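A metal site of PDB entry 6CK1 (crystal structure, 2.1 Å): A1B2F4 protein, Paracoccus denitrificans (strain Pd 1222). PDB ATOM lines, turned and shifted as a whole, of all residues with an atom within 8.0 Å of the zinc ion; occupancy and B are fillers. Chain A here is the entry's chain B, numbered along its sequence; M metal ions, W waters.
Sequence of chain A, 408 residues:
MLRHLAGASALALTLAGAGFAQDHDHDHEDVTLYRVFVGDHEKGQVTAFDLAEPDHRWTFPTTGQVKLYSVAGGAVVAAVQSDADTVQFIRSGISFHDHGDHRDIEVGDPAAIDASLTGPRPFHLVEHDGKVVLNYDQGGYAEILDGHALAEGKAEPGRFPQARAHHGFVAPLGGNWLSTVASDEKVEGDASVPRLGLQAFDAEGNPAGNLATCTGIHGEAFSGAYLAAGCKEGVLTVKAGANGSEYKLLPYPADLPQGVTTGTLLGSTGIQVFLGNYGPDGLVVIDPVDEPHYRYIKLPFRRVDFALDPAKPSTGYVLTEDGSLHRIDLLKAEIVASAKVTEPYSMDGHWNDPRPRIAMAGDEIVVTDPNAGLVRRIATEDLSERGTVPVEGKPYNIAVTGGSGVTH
The zinc ion is bound by NE2 of His 167 (2.0 Å), NE2 of His 124 (2.2 Å), NE2 of His 218 (2.3 Å) and water W1 (2.5 Å).
The nearest printed residue that does not touch the zinc ion is Phe 123 (4.2 Å).
O of Gly 263 is in hydrogen-bond range of ND1 of His 218, 2.6 Å away.
A ring nitrogen (ND1) of His 167 sits at hydrogen-bond distance from the side-chain carboxylate (OD2) of Asp 137 (2.5 Å).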
ATOM      1  N   PHE A 123     -15.038 -16.509  27.140  1.00  0.00           N
ATOM      2  CA  PHE A 123     -16.088 -16.672  28.124  1.00  0.00           C
ATOM      3  C   PHE A 123     -16.519 -18.137  28.260  1.00  0.00           C
ATOM      4  O   PHE A 123     -15.919 -18.887  29.040  1.00  0.00           O
ATOM      5  CB  PHE A 123     -17.276 -15.757  27.776  1.00  0.00           C
ATOM      6  CG  PHE A 123     -18.094 -15.389  28.962  1.00  0.00           C
ATOM      7  CD1 PHE A 123     -18.783 -16.343  29.663  1.00  0.00           C
ATOM      8  CD2 PHE A 123     -18.193 -14.060  29.383  1.00  0.00           C
ATOM      9  CE1 PHE A 123     -19.555 -16.000  30.764  1.00  0.00           C
ATOM     10  CE2 PHE A 123     -18.959 -13.706  30.484  1.00  0.00           C
ATOM     11  CZ  PHE A 123     -19.639 -14.688  31.175  1.00  0.00           C
ATOM     12  N   HIS A 124     -17.529 -18.573  27.517  1.00  0.00           N
ATOM     13  CA  HIS A 124     -18.064 -19.902  27.783  1.00  0.00           C
ATOM     14  C   HIS A 124     -17.107 -21.004  27.352  1.00  0.00           C
ATOM     15  O   HIS A 124     -16.481 -20.948  26.280  1.00  0.00           O
ATOM     16  CB  HIS A 124     -19.432 -20.093  27.134  1.00  0.00           C
ATOM     17  CG  HIS A 124     -20.537 -19.522  27.967  1.00  0.00           C
ATOM     18  ND1 HIS A 124     -20.845 -19.992  29.223  1.00  0.00           N
ATOM     19  CD2 HIS A 124     -21.381 -18.490  27.739  1.00  0.00           C
ATOM     20  CE1 HIS A 124     -21.837 -19.281  29.741  1.00  0.00           C
ATOM     21  NE2 HIS A 124     -22.189 -18.367  28.844  1.00  0.00           N
ATOM     22  N   ASP A 137     -15.969 -14.004  22.904  1.00  0.00           N
ATOM     23  CA  ASP A 137     -17.179 -13.233  22.649  1.00  0.00           C
ATOM     24  C   ASP A 137     -16.923 -12.045  21.734  1.00  0.00           C
ATOM     25  O   ASP A 137     -17.840 -11.593  21.046  1.00  0.00           O
ATOM     26  CB  ASP A 137     -17.781 -12.739  23.962  1.00  0.00           C
ATOM     27  CG  ASP A 137     -18.450 -13.827  24.745  1.00  0.00           C
ATOM     28  OD1 ASP A 137     -18.459 -15.000  24.290  1.00  0.00           O
ATOM     29  OD2 ASP A 137     -18.986 -13.516  25.832  1.00  0.00           O
ATOM     30  N   HIS A 167     -21.789 -13.567  22.204  1.00  0.00           N
ATOM     31  CA  HIS A 167     -21.698 -14.299  23.472  1.00  0.00           C
ATOM     32  C   HIS A 167     -22.310 -15.678  23.247  1.00  0.00           C
ATOM     33  O   HIS A 167     -23.519 -15.876  23.355  1.00  0.00           O
ATOM     34  CB  HIS A 167     -22.390 -13.538  24.597  1.00  0.00           C
ATOM     35  CG  HIS A 167     -22.358 -14.255  25.909  1.00  0.00           C
ATOM     36  ND1 HIS A 167     -21.179 -14.475  26.600  1.00  0.00           N
ATOM     37  CD2 HIS A 167     -23.333 -14.852  26.632  1.00  0.00           C
ATOM     38  CE1 HIS A 167     -21.443 -15.146  27.711  1.00  0.00           C
ATOM     39  NE2 HIS A 167     -22.740 -15.390  27.749  1.00  0.00           N
ATOM     40  N   GLY A 168     -21.462 -16.643  22.888  1.00  0.00           N
ATOM     41  CA  GLY A 168     -21.968 -17.936  22.505  1.00  0.00           C
ATOM     42  C   GLY A 168     -21.128 -19.052  23.049  1.00  0.00           C
ATOM     43  O   GLY A 168     -20.391 -18.874  24.033  1.00  0.00           O
ATOM     44  N   PHE A 169     -21.252 -20.234  22.446  1.00  0.00           N
ATOM     45  CA  PHE A 169     -20.462 -21.393  22.829  1.00  0.00           C
ATOM     46  C   PHE A 169     -20.325 -22.307  21.614  1.00  0.00           C
ATOM     47  O   PHE A 169     -21.128 -22.236  20.681  1.00  0.00           O
ATOM     48  CB  PHE A 169     -21.105 -22.140  24.013  1.00  0.00           C
ATOM     49  CG  PHE A 169     -22.470 -22.757  23.696  1.00  0.00           C
ATOM     50  CD1 PHE A 169     -22.570 -23.925  22.944  1.00  0.00           C
ATOM     51  CD2 PHE A 169     -23.636 -22.190  24.175  1.00  0.00           C
ATOM     52  CE1 PHE A 169     -23.803 -24.511  22.687  1.00  0.00           C
ATOM     53  CE2 PHE A 169     -24.885 -22.760  23.929  1.00  0.00           C
ATOM     54  CZ  PHE A 169     -24.966 -23.898  23.187  1.00  0.00           C
ATOM     55  N   ARG A 195     -28.928 -13.407  18.913  1.00  0.00           N
ATOM     56  CA  ARG A 195     -28.497 -14.720  18.488  1.00  0.00           C
ATOM     57  C   ARG A 195     -29.666 -15.515  17.896  1.00  0.00           C
ATOM     58  O   ARG A 195     -30.772 -15.506  18.437  1.00  0.00           O
ATOM     59  CB  ARG A 195     -27.886 -15.478  19.674  1.00  0.00           C
ATOM     60  CG  ARG A 195     -26.738 -14.710  20.342  1.00  0.00           C
ATOM     61  CD  ARG A 195     -26.129 -15.532  21.478  1.00  0.00           C
ATOM     62  NE  ARG A 195     -27.076 -15.680  22.580  1.00  0.00           N
ATOM     63  CZ  ARG A 195     -27.248 -14.773  23.522  1.00  0.00           C
ATOM     64  NH1 ARG A 195     -28.132 -14.980  24.501  1.00  0.00           N
ATOM     65  NH2 ARG A 195     -26.515 -13.645  23.502  1.00  0.00           N
ATOM     66  N   ILE A 217     -30.187 -18.030  22.103  1.00  0.00           N
ATOM     67  CA  ILE A 217     -29.643 -19.274  22.644  1.00  0.00           C
ATOM     68  C   ILE A 217     -28.655 -18.981  23.774  1.00  0.00           C
ATOM     69  O   ILE A 217     -27.715 -18.182  23.625  1.00  0.00           O
ATOM     70  CB  ILE A 217     -28.995 -20.139  21.546  1.00  0.00           C
ATOM     71  CG1 ILE A 217     -28.345 -21.395  22.120  1.00  0.00           C
ATOM     72  CG2 ILE A 217     -27.979 -19.355  20.665  1.00  0.00           C
ATOM     73  CD1 ILE A 217     -28.159 -22.464  21.024  1.00  0.00           C
ATOM     74  N   HIS A 218     -28.864 -19.630  24.914  1.00  0.00           N
ATOM     75  CA  HIS A 218     -28.016 -19.385  26.066  1.00  0.00           C
ATOM     76  C   HIS A 218     -28.095 -20.573  27.003  1.00  0.00           C
ATOM     77  O   HIS A 218     -29.180 -21.122  27.247  1.00  0.00           O
ATOM     78  CB  HIS A 218     -28.425 -18.104  26.822  1.00  0.00           C
ATOM     79  CG  HIS A 218     -27.414 -17.677  27.820  1.00  0.00           C
ATOM     80  ND1 HIS A 218     -27.305 -18.245  29.075  1.00  0.00           N
ATOM     81  CD2 HIS A 218     -26.412 -16.765  27.743  1.00  0.00           C
ATOM     82  CE1 HIS A 218     -26.299 -17.699  29.720  1.00  0.00           C
ATOM     83  NE2 HIS A 218     -25.746 -16.790  28.942  1.00  0.00           N
ATOM     84  N   GLY A 219     -26.943 -20.966  27.534  1.00  0.00           N
ATOM     85  CA  GLY A 219     -26.853 -22.106  28.416  1.00  0.00           C
ATOM     86  C   GLY A 219     -26.740 -23.421  27.659  1.00  0.00           C
ATOM     87  O   GLY A 219     -27.367 -23.623  26.616  1.00  0.00           O
ATOM     88  N   GLY A 263     -31.949 -20.349  30.873  1.00  0.00           N
ATOM     89  CA  GLY A 263     -30.723 -19.858  30.273  1.00  0.00           C
ATOM     90  C   GLY A 263     -29.456 -20.449  30.885  1.00  0.00           C
ATOM     91  O   GLY A 263     -28.360 -20.108  30.467  1.00  0.00           O
ATOM     92  N   THR A 264     -29.605 -21.323  31.881  1.00  0.00           N
ATOM     93  CA  THR A 264     -28.496 -21.999  32.551  1.00  0.00           C
ATOM     94  C   THR A 264     -28.880 -23.462  32.746  1.00  0.00           C
ATOM     95  O   THR A 264     -29.966 -23.748  33.249  1.00  0.00           O
ATOM     96  CB  THR A 264     -28.188 -21.358  33.912  1.00  0.00           C
ATOM     97  OG1 THR A 264     -27.979 -19.949  33.743  1.00  0.00           O
ATOM     98  CG2 THR A 264     -26.917 -22.012  34.568  1.00  0.00           C
ATOM     99  N   TRP A 351     -25.042  -9.135  37.687  1.00  0.00           N
ATOM    100  CA  TRP A 351     -24.934 -10.586  37.774  1.00  0.00           C
ATOM    101  C   TRP A 351     -23.573 -11.037  38.290  1.00  0.00           C
ATOM    102  O   TRP A 351     -23.462 -12.143  38.824  1.00  0.00           O
ATOM    103  CB  TRP A 351     -25.221 -11.238  36.414  1.00  0.00           C
ATOM    104  CG  TRP A 351     -24.180 -10.913  35.399  1.00  0.00           C
ATOM    105  CD1 TRP A 351     -24.207  -9.867  34.523  1.00  0.00           C
ATOM    106  CD2 TRP A 351     -22.942 -11.603  35.177  1.00  0.00           C
ATOM    107  NE1 TRP A 351     -23.061  -9.872  33.758  1.00  0.00           N
ATOM    108  CE2 TRP A 351     -22.269 -10.929  34.130  1.00  0.00           C
ATOM    109  CE3 TRP A 351     -22.335 -12.726  35.761  1.00  0.00           C
ATOM    110  CZ2 TRP A 351     -21.006 -11.338  33.659  1.00  0.00           C
ATOM    111  CZ3 TRP A 351     -21.093 -13.133  35.283  1.00  0.00           C
ATOM    112  CH2 TRP A 351     -20.450 -12.444  34.246  1.00  0.00           C
HETATM  113 ZN    ZN M   1     -23.428 -16.565  29.206  1.00  0.00          ZN
HETATM  114  O   HOH W   1     -23.350 -15.802  31.538  1.00  0.00           O
